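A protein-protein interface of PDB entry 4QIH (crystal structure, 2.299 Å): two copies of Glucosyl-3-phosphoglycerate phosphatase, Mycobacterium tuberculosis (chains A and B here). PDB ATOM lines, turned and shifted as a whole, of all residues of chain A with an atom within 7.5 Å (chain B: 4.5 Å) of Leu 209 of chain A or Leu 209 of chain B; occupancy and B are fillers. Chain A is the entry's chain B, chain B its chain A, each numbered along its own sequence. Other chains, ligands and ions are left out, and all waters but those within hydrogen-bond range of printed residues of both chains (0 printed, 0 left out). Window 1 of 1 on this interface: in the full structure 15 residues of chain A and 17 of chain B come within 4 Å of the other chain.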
ATOM      1  N   MET A   8     -24.489   2.233  34.675  1.00  0.00           N
ATOM      2  CA  MET A   8     -23.554   1.632  35.623  1.00  0.00           C
ATOM      3  C   MET A   8     -22.119   2.025  35.234  1.00  0.00           C
ATOM      4  O   MET A   8     -21.685   1.789  34.107  1.00  0.00           O
ATOM      5  CB  MET A   8     -23.718   0.106  35.654  1.00  0.00           C
ATOM      6  CG  MET A   8     -24.966  -0.367  36.354  1.00  0.00           C
ATOM      7  SD  MET A   8     -25.182  -2.157  36.238  1.00  0.00           S
ATOM      8  CE  MET A   8     -25.733  -2.182  34.530  1.00  0.00           C
ATOM      9  N   ARG A 110     -12.830 -16.795  35.181  1.00  0.00           N
ATOM     10  CA  ARG A 110     -13.540 -15.876  34.271  1.00  0.00           C
ATOM     11  C   ARG A 110     -14.647 -16.585  33.486  1.00  0.00           C
ATOM     12  O   ARG A 110     -15.656 -15.987  33.143  1.00  0.00           O
ATOM     13  CB  ARG A 110     -12.584 -15.210  33.268  1.00  0.00           C
ATOM     14  CG  ARG A 110     -12.920 -13.764  33.031  1.00  0.00           C
ATOM     15  CD  ARG A 110     -12.583 -13.282  31.613  1.00  0.00           C
ATOM     16  NE  ARG A 110     -13.395 -13.988  30.625  1.00  0.00           N
ATOM     17  CZ  ARG A 110     -14.610 -13.616  30.211  1.00  0.00           C
ATOM     18  NH1 ARG A 110     -15.183 -12.495  30.649  1.00  0.00           N
ATOM     19  NH2 ARG A 110     -15.245 -14.369  29.324  1.00  0.00           N
ATOM     20  N   SER A 167     -25.640  -6.899  35.552  1.00  0.00           N
ATOM     21  CA  SER A 167     -26.170  -6.745  34.184  1.00  0.00           C
ATOM     22  C   SER A 167     -26.663  -8.088  33.652  1.00  0.00           C
ATOM     23  O   SER A 167     -27.780  -8.189  33.128  1.00  0.00           O
ATOM     24  CB  SER A 167     -25.098  -6.170  33.235  1.00  0.00           C
ATOM     25  OG  SER A 167     -24.791  -4.816  33.526  1.00  0.00           O
ATOM     26  N   LEU A 171     -30.504  -8.929  32.617  1.00  0.00           N
ATOM     27  CA  LEU A 171     -30.837  -9.397  31.271  1.00  0.00           C
ATOM     28  C   LEU A 171     -31.462 -10.783  31.274  1.00  0.00           C
ATOM     29  O   LEU A 171     -31.982 -11.234  30.256  1.00  0.00           O
ATOM     30  CB  LEU A 171     -29.576  -9.387  30.399  1.00  0.00           C
ATOM     31  CG  LEU A 171     -29.006  -7.969  30.198  1.00  0.00           C
ATOM     32  CD1 LEU A 171     -27.693  -8.051  29.557  1.00  0.00           C
ATOM     33  CD2 LEU A 171     -29.920  -7.095  29.343  1.00  0.00           C
ATOM     34  N   PRO A 179     -20.341 -15.223  31.286  1.00  0.00           N
ATOM     35  CA  PRO A 179     -18.990 -14.801  30.867  1.00  0.00           C
ATOM     36  C   PRO A 179     -18.959 -14.126  29.472  1.00  0.00           C
ATOM     37  O   PRO A 179     -17.903 -13.688  29.007  1.00  0.00           O
ATOM     38  CB  PRO A 179     -18.200 -16.119  30.844  1.00  0.00           C
ATOM     39  CG  PRO A 179     -18.961 -17.029  31.773  1.00  0.00           C
ATOM     40  CD  PRO A 179     -20.403 -16.679  31.478  1.00  0.00           C
ATOM     41  N   ALA A 180     -20.118 -14.008  28.836  1.00  0.00           N
ATOM     42  CA  ALA A 180     -20.230 -13.340  27.547  1.00  0.00           C
ATOM     43  C   ALA A 180     -19.858 -11.860  27.688  1.00  0.00           C
ATOM     44  O   ALA A 180     -19.352 -11.235  26.762  1.00  0.00           O
ATOM     45  CB  ALA A 180     -21.644 -13.512  26.992  1.00  0.00           C
ATOM     46  N   LEU A 181     -20.061 -11.318  28.871  1.00  0.00           N
ATOM     47  CA  LEU A 181     -19.762  -9.913  29.123  1.00  0.00           C
ATOM     48  C   LEU A 181     -18.303  -9.656  29.532  1.00  0.00           C
ATOM     49  O   LEU A 181     -17.846 -10.130  30.555  1.00  0.00           O
ATOM     50  CB  LEU A 181     -20.693  -9.383  30.202  1.00  0.00           C
ATOM     51  CG  LEU A 181     -22.180  -9.479  29.874  1.00  0.00           C
ATOM     52  CD1 LEU A 181     -23.029  -8.835  31.012  1.00  0.00           C
ATOM     53  CD2 LEU A 181     -22.485  -8.832  28.550  1.00  0.00           C
ATOM     54  N   GLY A 182     -17.586  -8.897  28.719  1.00  0.00           N
ATOM     55  CA  GLY A 182     -16.191  -8.638  28.979  1.00  0.00           C
ATOM     56  C   GLY A 182     -15.985  -7.477  29.920  1.00  0.00           C
ATOM     57  O   GLY A 182     -16.843  -6.619  30.080  1.00  0.00           O
ATOM     58  N   GLY A 183     -14.794  -7.414  30.478  1.00  0.00           N
ATOM     59  CA  GLY A 183     -14.476  -6.483  31.538  1.00  0.00           C
ATOM     60  C   GLY A 183     -14.567  -5.034  31.126  1.00  0.00           C
ATOM     61  O   GLY A 183     -14.085  -4.622  30.075  1.00  0.00           O
ATOM     62  N   MET A 184     -15.193  -4.254  31.984  1.00  0.00           N
ATOM     63  CA  MET A 184     -15.354  -2.839  31.747  1.00  0.00           C
ATOM     64  C   MET A 184     -14.042  -2.089  31.900  1.00  0.00           C
ATOM     65  O   MET A 184     -13.271  -2.390  32.792  1.00  0.00           O
ATOM     66  CB  MET A 184     -16.348  -2.252  32.731  1.00  0.00           C
ATOM     67  CG  MET A 184     -17.668  -2.959  32.794  1.00  0.00           C
ATOM     68  SD  MET A 184     -18.934  -2.122  31.859  1.00  0.00           S
ATOM     69  CE  MET A 184     -19.021  -0.523  32.675  1.00  0.00           C
ATOM     70  N   THR A 190     -22.042   1.483  31.266  1.00  0.00           N
ATOM     71  CA  THR A 190     -22.959   0.558  30.601  1.00  0.00           C
ATOM     72  C   THR A 190     -24.366   1.043  30.779  1.00  0.00           C
ATOM     73  O   THR A 190     -24.669   1.632  31.797  1.00  0.00           O
ATOM     74  CB  THR A 190     -22.802  -0.860  31.178  1.00  0.00           C
ATOM     75  OG1 THR A 190     -21.617  -1.430  30.619  1.00  0.00           O
ATOM     76  CG2 THR A 190     -23.991  -1.780  30.897  1.00  0.00           C
ATOM     77  N   GLN A 191     -25.228   0.835  29.788  1.00  0.00           N
ATOM     78  CA  GLN A 191     -26.603   1.246  29.955  1.00  0.00           C
ATOM     79  C   GLN A 191     -27.549   0.120  29.655  1.00  0.00           C
ATOM     80  O   GLN A 191     -27.473  -0.521  28.606  1.00  0.00           O
ATOM     81  CB  GLN A 191     -26.959   2.441  29.077  1.00  0.00           C
ATOM     82  CG  GLN A 191     -28.420   2.827  29.310  1.00  0.00           C
ATOM     83  CD  GLN A 191     -28.870   4.019  28.528  1.00  0.00           C
ATOM     84  OE1 GLN A 191     -28.396   5.133  28.726  1.00  0.00           O
ATOM     85  NE2 GLN A 191     -29.794   3.789  27.620  1.00  0.00           N
ATOM     86  N   LEU A 192     -28.455  -0.095  30.599  1.00  0.00           N
ATOM     87  CA  LEU A 192     -29.556  -1.022  30.414  1.00  0.00           C
ATOM     88  C   LEU A 192     -30.867  -0.254  30.368  1.00  0.00           C
ATOM     89  O   LEU A 192     -31.028   0.800  31.018  1.00  0.00           O
ATOM     90  CB  LEU A 192     -29.590  -2.034  31.534  1.00  0.00           C
ATOM     91  CG  LEU A 192     -28.881  -3.366  31.344  1.00  0.00           C
ATOM     92  CD1 LEU A 192     -27.532  -3.207  30.758  1.00  0.00           C
ATOM     93  CD2 LEU A 192     -28.775  -4.045  32.696  1.00  0.00           C
ATOM     94  N   SER A 193     -31.810  -0.812  29.619  1.00  0.00           N
ATOM     95  CA  SER A 193     -33.164  -0.301  29.571  1.00  0.00           C
ATOM     96  C   SER A 193     -34.154  -1.364  30.041  1.00  0.00           C
ATOM     97  O   SER A 193     -34.158  -2.477  29.529  1.00  0.00           O
ATOM     98  CB  SER A 193     -33.514   0.159  28.150  1.00  0.00           C
ATOM     99  OG  SER A 193     -33.126   1.509  27.957  1.00  0.00           O
ATOM    100  N   HIS A 195     -38.006  -2.319  30.252  1.00  0.00           N
ATOM    101  CA  HIS A 195     -39.308  -2.045  29.652  1.00  0.00           C
ATOM    102  C   HIS A 195     -40.467  -2.732  30.379  1.00  0.00           C
ATOM    103  O   HIS A 195     -41.513  -2.120  30.596  1.00  0.00           O
ATOM    104  CB  HIS A 195     -39.286  -2.479  28.191  1.00  0.00           C
ATOM    105  CG  HIS A 195     -38.203  -1.826  27.386  1.00  0.00           C
ATOM    106  ND1 HIS A 195     -38.457  -0.819  26.474  1.00  0.00           N
ATOM    107  CD2 HIS A 195     -36.864  -2.035  27.355  1.00  0.00           C
ATOM    108  CE1 HIS A 195     -37.321  -0.439  25.916  1.00  0.00           C
ATOM    109  NE2 HIS A 195     -36.339  -1.158  26.432  1.00  0.00           N
ATOM    110  N   TRP A 207     -35.221  -6.282  30.669  1.00  0.00           N
ATOM    111  CA  TRP A 207     -34.074  -5.413  30.488  1.00  0.00           C
ATOM    112  C   TRP A 207     -33.392  -5.732  29.185  1.00  0.00           C
ATOM    113  O   TRP A 207     -33.303  -6.884  28.788  1.00  0.00           O
ATOM    114  CB  TRP A 207     -33.101  -5.584  31.653  1.00  0.00           C
ATOM    115  CG  TRP A 207     -33.743  -5.175  32.926  1.00  0.00           C
ATOM    116  CD1 TRP A 207     -34.474  -5.968  33.761  1.00  0.00           C
ATOM    117  CD2 TRP A 207     -33.758  -3.857  33.503  1.00  0.00           C
ATOM    118  NE1 TRP A 207     -34.921  -5.235  34.833  1.00  0.00           N
ATOM    119  CE2 TRP A 207     -34.493  -3.941  34.702  1.00  0.00           C
ATOM    120  CE3 TRP A 207     -33.204  -2.627  33.128  1.00  0.00           C
ATOM    121  CZ2 TRP A 207     -34.695  -2.848  35.527  1.00  0.00           C
ATOM    122  CZ3 TRP A 207     -33.398  -1.530  33.949  1.00  0.00           C
ATOM    123  CH2 TRP A 207     -34.139  -1.649  35.143  1.00  0.00           C
ATOM    124  N   ARG A 208     -32.917  -4.703  28.518  1.00  0.00           N
ATOM    125  CA  ARG A 208     -32.058  -4.885  27.359  1.00  0.00           C
ATOM    126  C   ARG A 208     -30.824  -4.015  27.472  1.00  0.00           C
ATOM    127  O   ARG A 208     -30.814  -3.009  28.182  1.00  0.00           O
ATOM    128  CB  ARG A 208     -32.820  -4.578  26.077  1.00  0.00           C
ATOM    129  CG  ARG A 208     -33.032  -3.084  25.822  1.00  0.00           C
ATOM    130  CD  ARG A 208     -34.093  -2.871  24.737  1.00  0.00           C
ATOM    131  NE  ARG A 208     -35.329  -3.616  25.024  1.00  0.00           N
ATOM    132  CZ  ARG A 208     -36.507  -3.407  24.430  1.00  0.00           C
ATOM    133  NH1 ARG A 208     -36.629  -2.459  23.506  1.00  0.00           N
ATOM    134  NH2 ARG A 208     -37.574  -4.149  24.770  1.00  0.00           N
ATOM    135  N   LEU A 209     -29.795  -4.408  26.736  1.00  0.00           N
ATOM    136  CA  LEU A 209     -28.524  -3.738  26.780  1.00  0.00           C
ATOM    137  C   LEU A 209     -28.436  -2.669  25.707  1.00  0.00           C
ATOM    138  O   LEU A 209     -28.462  -2.981  24.520  1.00  0.00           O
ATOM    139  CB  LEU A 209     -27.420  -4.778  26.604  1.00  0.00           C
ATOM    140  CG  LEU A 209     -25.972  -4.276  26.548  1.00  0.00           C
ATOM    141  CD1 LEU A 209     -25.474  -3.826  27.920  1.00  0.00           C
ATOM    142  CD2 LEU A 209     -25.114  -5.343  25.995  1.00  0.00           C
ATOM    143  N   ASP A 210     -28.365  -1.409  26.103  1.00  0.00           N
ATOM    144  CA  ASP A 210     -28.214  -0.330  25.134  1.00  0.00           C
ATOM    145  C   ASP A 210     -26.741  -0.046  24.843  1.00  0.00           C
ATOM    146  O   ASP A 210     -26.371   0.283  23.730  1.00  0.00           O
ATOM    147  CB  ASP A 210     -28.858   0.973  25.627  1.00  0.00           C
ATOM    148  CG  ASP A 210     -30.300   0.804  26.002  1.00  0.00           C
ATOM    149  OD1 ASP A 210     -31.026   0.008  25.353  1.00  0.00           O
ATOM    150  OD2 ASP A 210     -30.695   1.467  26.979  1.00  0.00           O
ATOM    151  N   VAL A 211     -25.917  -0.124  25.867  1.00  0.00           N
ATOM    152  CA  VAL A 211     -24.516   0.273  25.761  1.00  0.00           C
ATOM    153  C   VAL A 211     -23.725  -0.629  26.663  1.00  0.00           C
ATOM    154  O   VAL A 211     -24.136  -0.824  27.798  1.00  0.00           O
ATOM    155  CB  VAL A 211     -24.299   1.732  26.201  1.00  0.00           C
ATOM    156  CG1 VAL A 211     -22.800   2.086  26.296  1.00  0.00           C
ATOM    157  CG2 VAL A 211     -25.017   2.699  25.285  1.00  0.00           C
ATOM    158  N   TRP A 212     -22.652  -1.231  26.158  1.00  0.00           N
ATOM    159  CA  TRP A 212     -21.698  -1.944  27.033  1.00  0.00           C
ATOM    160  C   TRP A 212     -20.263  -1.374  26.874  1.00  0.00           C
ATOM    161  O   TRP A 212     -19.671  -1.465  25.806  1.00  0.00           O
ATOM    162  CB  TRP A 212     -21.704  -3.478  26.780  1.00  0.00           C
ATOM    163  CG  TRP A 212     -20.758  -4.222  27.704  1.00  0.00           C
ATOM    164  CD1 TRP A 212     -19.526  -4.676  27.399  1.00  0.00           C
ATOM    165  CD2 TRP A 212     -20.965  -4.535  29.096  1.00  0.00           C
ATOM    166  NE1 TRP A 212     -18.949  -5.286  28.498  1.00  0.00           N
ATOM    167  CE2 TRP A 212     -19.812  -5.203  29.552  1.00  0.00           C
ATOM    168  CE3 TRP A 212     -22.016  -4.324  29.995  1.00  0.00           C
ATOM    169  CZ2 TRP A 212     -19.676  -5.656  30.865  1.00  0.00           C
ATOM    170  CZ3 TRP A 212     -21.889  -4.776  31.288  1.00  0.00           C
ATOM    171  CH2 TRP A 212     -20.722  -5.438  31.720  1.00  0.00           C
ATOM    172  N   ASN A 213     -19.734  -0.793  27.953  1.00  0.00           N
ATOM    173  CA  ASN A 213     -18.327  -0.392  28.064  1.00  0.00           C
ATOM    174  C   ASN A 213     -17.997   0.747  27.119  1.00  0.00           C
ATOM    175  O   ASN A 213     -17.036   0.671  26.370  1.00  0.00           O
ATOM    176  CB  ASN A 213     -17.418  -1.588  27.781  1.00  0.00           C
ATOM    177  CG  ASN A 213     -15.988  -1.394  28.300  1.00  0.00           C
ATOM    178  OD1 ASN A 213     -15.760  -0.670  29.273  1.00  0.00           O
ATOM    179  ND2 ASN A 213     -15.019  -2.042  27.638  1.00  0.00           N
ATOM    180  N   LEU B 171     -21.789 -15.051  20.277  1.00  0.00           N
ATOM    181  CA  LEU B 171     -21.753 -15.254  21.708  1.00  0.00           C
ATOM    182  C   LEU B 171     -22.435 -16.563  22.159  1.00  0.00           C
ATOM    183  O   LEU B 171     -22.331 -16.928  23.307  1.00  0.00           O
ATOM    184  CB  LEU B 171     -22.425 -14.096  22.419  1.00  0.00           C
ATOM    185  CG  LEU B 171     -21.721 -12.773  22.224  1.00  0.00           C
ATOM    186  CD1 LEU B 171     -22.609 -11.708  22.815  1.00  0.00           C
ATOM    187  CD2 LEU B 171     -20.356 -12.765  22.894  1.00  0.00           C
ATOM    188  N   ALA B 180     -31.897  -9.501  24.349  1.00  0.00           N
ATOM    189  CA  ALA B 180     -31.155  -8.766  25.351  1.00  0.00           C
ATOM    190  C   ALA B 180     -30.262  -7.691  24.669  1.00  0.00           C
ATOM    191  O   ALA B 180     -29.972  -6.632  25.244  1.00  0.00           O
ATOM    192  CB  ALA B 180     -30.351  -9.719  26.176  1.00  0.00           C
ATOM    193  N   LEU B 181     -29.874  -7.936  23.419  1.00  0.00           N
ATOM    194  CA  LEU B 181     -29.051  -6.960  22.694  1.00  0.00           C
ATOM    195  C   LEU B 181     -29.904  -5.916  22.004  1.00  0.00           C
ATOM    196  O   LEU B 181     -30.771  -6.208  21.166  1.00  0.00           O
ATOM    197  CB  LEU B 181     -28.116  -7.635  21.693  1.00  0.00           C
ATOM    198  CG  LEU B 181     -27.141  -8.600  22.378  1.00  0.00           C
ATOM    199  CD1 LEU B 181     -26.193  -9.198  21.365  1.00  0.00           C
ATOM    200  CD2 LEU B 181     -26.362  -7.894  23.483  1.00  0.00           C
ATOM    201  N   GLY B 182     -29.592  -4.691  22.399  1.00  0.00           N
ATOM    202  CA  GLY B 182     -30.299  -3.484  22.046  1.00  0.00           C
ATOM    203  C   GLY B 182     -29.952  -2.916  20.708  1.00  0.00           C
ATOM    204  O   GLY B 182     -29.651  -3.640  19.761  1.00  0.00           O
ATOM    205  N   GLY B 183     -30.138  -1.605  20.637  1.00  0.00           N
ATOM    206  CA  GLY B 183     -30.033  -0.847  19.421  1.00  0.00           C
ATOM    207  C   GLY B 183     -28.761  -0.025  19.315  1.00  0.00           C
ATOM    208  O   GLY B 183     -28.409   0.760  20.197  1.00  0.00           O
ATOM    209  N   THR B 190     -19.500  -2.074  17.705  1.00  0.00           N
ATOM    210  CA  THR B 190     -19.491  -3.133  18.701  1.00  0.00           C
ATOM    211  C   THR B 190     -18.237  -3.956  18.414  1.00  0.00           C
ATOM    212  O   THR B 190     -17.851  -4.086  17.255  1.00  0.00           O
ATOM    213  CB  THR B 190     -20.752  -3.983  18.619  1.00  0.00           C
ATOM    214  OG1 THR B 190     -21.815  -3.268  19.250  1.00  0.00           O
ATOM    215  CG2 THR B 190     -20.600  -5.375  19.262  1.00  0.00           C
ATOM    216  N   GLN B 191     -17.597  -4.457  19.470  1.00  0.00           N
ATOM    217  CA  GLN B 191     -16.410  -5.312  19.356  1.00  0.00           C
ATOM    218  C   GLN B 191     -16.590  -6.573  20.173  1.00  0.00           C
ATOM    219  O   GLN B 191     -16.954  -6.519  21.343  1.00  0.00           O
ATOM    220  CB  GLN B 191     -15.148  -4.603  19.827  1.00  0.00           C
ATOM    221  CG  GLN B 191     -13.880  -5.469  19.797  1.00  0.00           C
ATOM    222  CD  GLN B 191     -12.652  -4.671  20.280  1.00  0.00           C
ATOM    223  OE1 GLN B 191     -12.291  -3.688  19.679  1.00  0.00           O
ATOM    224  NE2 GLN B 191     -12.042  -5.094  21.375  1.00  0.00           N
ATOM    225  N   LEU B 192     -16.322  -7.691  19.518  1.00  0.00           N
ATOM    226  CA  LEU B 192     -16.289  -8.964  20.131  1.00  0.00           C
ATOM    227  C   LEU B 192     -14.859  -9.447  20.071  1.00  0.00           C
ATOM    228  O   LEU B 192     -14.108  -9.065  19.198  1.00  0.00           O
ATOM    229  CB  LEU B 192     -17.224  -9.932  19.414  1.00  0.00           C
ATOM    230  CG  LEU B 192     -18.685 -10.038  19.900  1.00  0.00           C
ATOM    231  CD1 LEU B 192     -19.339  -8.734  20.106  1.00  0.00           C
ATOM    232  CD2 LEU B 192     -19.525 -10.836  18.918  1.00  0.00           C
ATOM    233  N   ARG B 208     -16.480 -13.121  23.365  1.00  0.00           N
ATOM    234  CA  ARG B 208     -17.061 -12.338  24.447  1.00  0.00           C
ATOM    235  C   ARG B 208     -17.316 -10.930  23.941  1.00  0.00           C
ATOM    236  O   ARG B 208     -16.779 -10.525  22.912  1.00  0.00           O
ATOM    237  CB  ARG B 208     -16.176 -12.300  25.688  1.00  0.00           C
ATOM    238  CG  ARG B 208     -15.013 -11.324  25.594  1.00  0.00           C
ATOM    239  CD  ARG B 208     -13.992 -11.448  26.724  1.00  0.00           C
ATOM    240  NE  ARG B 208     -13.441 -12.796  26.903  1.00  0.00           N
ATOM    241  CZ  ARG B 208     -12.336 -13.054  27.606  1.00  0.00           C
ATOM    242  NH1 ARG B 208     -11.692 -12.063  28.192  1.00  0.00           N
ATOM    243  NH2 ARG B 208     -11.868 -14.295  27.725  1.00  0.00           N
ATOM    244  N   LEU B 209     -18.169 -10.193  24.636  1.00  0.00           N
ATOM    245  CA  LEU B 209     -18.512  -8.826  24.210  1.00  0.00           C
ATOM    246  C   LEU B 209     -17.599  -7.800  24.891  1.00  0.00           C
ATOM    247  O   LEU B 209     -17.659  -7.631  26.115  1.00  0.00           O
ATOM    248  CB  LEU B 209     -20.001  -8.578  24.503  1.00  0.00           C
ATOM    249  CG  LEU B 209     -20.586  -7.192  24.242  1.00  0.00           C
ATOM    250  CD1 LEU B 209     -20.615  -6.908  22.776  1.00  0.00           C
ATOM    251  CD2 LEU B 209     -22.021  -7.172  24.796  1.00  0.00           C
ATOM    252  N   ASP B 210     -16.733  -7.125  24.123  1.00  0.00           N
ATOM    253  CA  ASP B 210     -15.827  -6.134  24.732  1.00  0.00           C
ATOM    254  C   ASP B 210     -16.502  -4.781  24.806  1.00  0.00           C
ATOM    255  O   ASP B 210     -16.302  -4.004  25.746  1.00  0.00           O
ATOM    256  CB  ASP B 210     -14.514  -5.973  23.959  1.00  0.00           C
ATOM    257  CG  ASP B 210     -13.759  -7.277  23.763  1.00  0.00           C
ATOM    258  OD1 ASP B 210     -13.758  -8.176  24.635  1.00  0.00           O
ATOM    259  OD2 ASP B 210     -13.157  -7.402  22.690  1.00  0.00           O
ATOM    260  N   VAL B 211     -17.258  -4.471  23.762  1.00  0.00           N
ATOM    261  CA  VAL B 211     -17.902  -3.180  23.685  1.00  0.00           C
ATOM    262  C   VAL B 211     -19.200  -3.354  22.923  1.00  0.00           C
ATOM    263  O   VAL B 211     -19.189  -3.929  21.852  1.00  0.00           O
ATOM    264  CB  VAL B 211     -17.017  -2.139  22.985  1.00  0.00           C
ATOM    265  CG1 VAL B 211     -17.780  -0.859  22.865  1.00  0.00           C
ATOM    266  CG2 VAL B 211     -15.667  -1.911  23.745  1.00  0.00           C
ATOM    267  N   TRP B 212     -20.298  -2.838  23.459  1.00  0.00           N
ATOM    268  CA  TRP B 212     -21.567  -2.769  22.716  1.00  0.00           C
ATOM    269  C   TRP B 212     -21.966  -1.303  22.540  1.00  0.00           C
ATOM    270  O   TRP B 212     -22.127  -0.583  23.517  1.00  0.00           O
ATOM    271  CB  TRP B 212     -22.721  -3.562  23.410  1.00  0.00           C
ATOM    272  CG  TRP B 212     -24.023  -3.435  22.627  1.00  0.00           C
ATOM    273  CD1 TRP B 212     -25.037  -2.557  22.868  1.00  0.00           C
ATOM    274  CD2 TRP B 212     -24.404  -4.180  21.466  1.00  0.00           C
ATOM    275  NE1 TRP B 212     -26.022  -2.702  21.920  1.00  0.00           N
ATOM    276  CE2 TRP B 212     -25.655  -3.691  21.045  1.00  0.00           C
ATOM    277  CE3 TRP B 212     -23.811  -5.228  20.747  1.00  0.00           C
ATOM    278  CZ2 TRP B 212     -26.328  -4.218  19.932  1.00  0.00           C
ATOM    279  CZ3 TRP B 212     -24.455  -5.746  19.666  1.00  0.00           C
ATOM    280  CH2 TRP B 212     -25.707  -5.240  19.251  1.00  0.00           C
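The backbone carbonyl oxygen (O) of Ala 180 of chain B lies within hydrogen-bond range of the backbone NH (N) of Leu 209 of chain A.
O of Leu 209 of chain A lies within hydrogen-bond range of N of Gly 182 of chain B.
The backbone NH (N) of Leu 209 of chain B lies within hydrogen-bond range of the backbone carbonyl oxygen (O) of Ala 180 of chain A, 2.6 Å away.
O of Leu 209 of chain B lies within hydrogen-bond range of N of Gly 182 of chain A (2.9 Å).
The side-chain amide nitrogen (ND2) of Asn 213 of chain A sits at hydrogen-bond distance from the backbone carbonyl oxygen (O) of Asp 210 of chain B (3.0 Å).
The backbone carbonyl oxygen (O) of Trp 212 of chain B sits at hydrogen-bond distance from the backbone NH (N) of Trp 212 of chain A, 2.8 Å away.
NE of Arg 110 of chain A lies close to NH2 of Arg 208 of chain B (3.3 Å).
O of Gln 191 of chain B sits at hydrogen-bond distance from N of Asp 210 of chain B, 2.9 Å away.
The backbone NH (N) of Gln 191 of chain B is in hydrogen-bond range of the backbone carbonyl oxygen (O) of Val 211 of chain B (2.9 Å).
The indole nitrogen (NE1) of Trp 212 of chain A lies within hydrogen-bond range of the backbone carbonyl oxygen (O) of Gly 182 of chain A, 3.0 Å away.
OD2 of Asp 210 of chain A lies within hydrogen-bond range of NE2 of Gln 191 of chain A (2.6 Å).
The backbone carbonyl oxygen of Ser 193 of chain A lies within hydrogen-bond range of the backbone NH of Arg 208 of chain A (2.7 Å).
NE2 of His 195 of chain A sits at hydrogen-bond distance from NE of Arg 208 of chain A (3.0 Å).
Among the printed residues, merely in contact across the chains: Trp 212 of chain A with Val 211 of chain B (3.3 Å), Asp 210 of chain A with Trp 212 of chain B (3.3 Å), Val 211 of chain A with Trp 212 of chain B (3.4 Å), Ala 180 of chain A with Arg 208 of chain B (3.4 Å), Arg 208 of chain A with Ala 180 of chain B (3.4 Å), Leu 209 of chain A with Trp 212 of chain B (3.6 Å), Trp 212 of chain A with Leu 209 of chain B (3.6 Å), Trp 212 of chain A with Asp 210 of chain B (3.7 Å), Leu 209 of chain A with Leu 209 of chain B (3.8 Å), Leu 209 of chain A with Leu 181 of chain B (3.8 Å), Asn 213 of chain A with Val 211 of chain B (3.9 Å) and Pro 179 of chain A with Arg 208 of chain B (3.99 Å).
Printed residues of chain B within 4 Å of Leu 209 of chain A: Ala 180 (2.7 Å), Leu 181 (3.8 Å), Gly 182 (2.9 Å), Leu 209 (3.8 Å) and Trp 212 (3.6 Å).
Of chain A, only Ala 180 (2.6 Å), Gly 182 (2.9 Å), Leu 209 (3.8 Å) and Trp 212 (3.6 Å) come within 4 Å of Leu 209 of chain B.
Of the printed residues of chain B, Asn 213 of chain A touches Asp 210 (3.0 Å) and Val 211 (3.9 Å).
Of the printed residues of chain B, Ala 180 of chain A touches Arg 208 and Leu 209.
Of the printed residues of chain A, Ala 180 of chain B touches Arg 208 (3.4 Å) and Leu 209 (2.7 Å).
Printed residues of chain A within 4 Å of Trp 212 of chain B: Leu 209 (3.6 Å), Asp 210 (3.3 Å), Val 211 (3.4 Å) and Trp 212 (2.8 Å).
Of the printed residues of chain A, Gly 182 of chain B touches Leu 209 (2.9 Å).
The nearest residue of chain A that does not touch Leu 209 of chain B is Leu 181 of chain A (4.02 Å).
The nearest printed residue of chain A that does not touch Arg 208 of chain B is Gly 182 of chain A (4.2 Å).
Hydrophobic or aromatic side chains of chain A within 4 Å of the printed part of chain B: Leu 209, Val 211 and Trp 212.
Of the 13 printed residues of chain B, 8 touch a printed residue of chain A.
Printed residues of chain B that touch a printed residue of chain A: Ala 180, Leu 181, Gly 182, Arg 208, Leu 209, Asp 210, Val 211 and Trp 212.
Among the printed residues, 19 pairs touch across the chains.
Among the printed residues, no Asp or Glu carboxylate lies within 4 Å of a Lys or Arg side-chain nitrogen of the other chain.
Leu 209 of chain A touches its own counterpart, Leu 209 of chain B.
Asp 210 of chain A touches Trp 212 of chain B, and with the chains exchanged Trp 212 of chain A touches Asp 210 of chain B.
Val 211 of chain A touches Trp 212 of chain B, and with the chains exchanged Trp 212 of chain A touches Val 211 of chain B.
Trp 212 of chain B touches its own counterpart, Trp 212 of chain A.
Of the 19 pairs that touch across the chains among the printed residues, 14 have their exchanged pair printed and touching as well.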
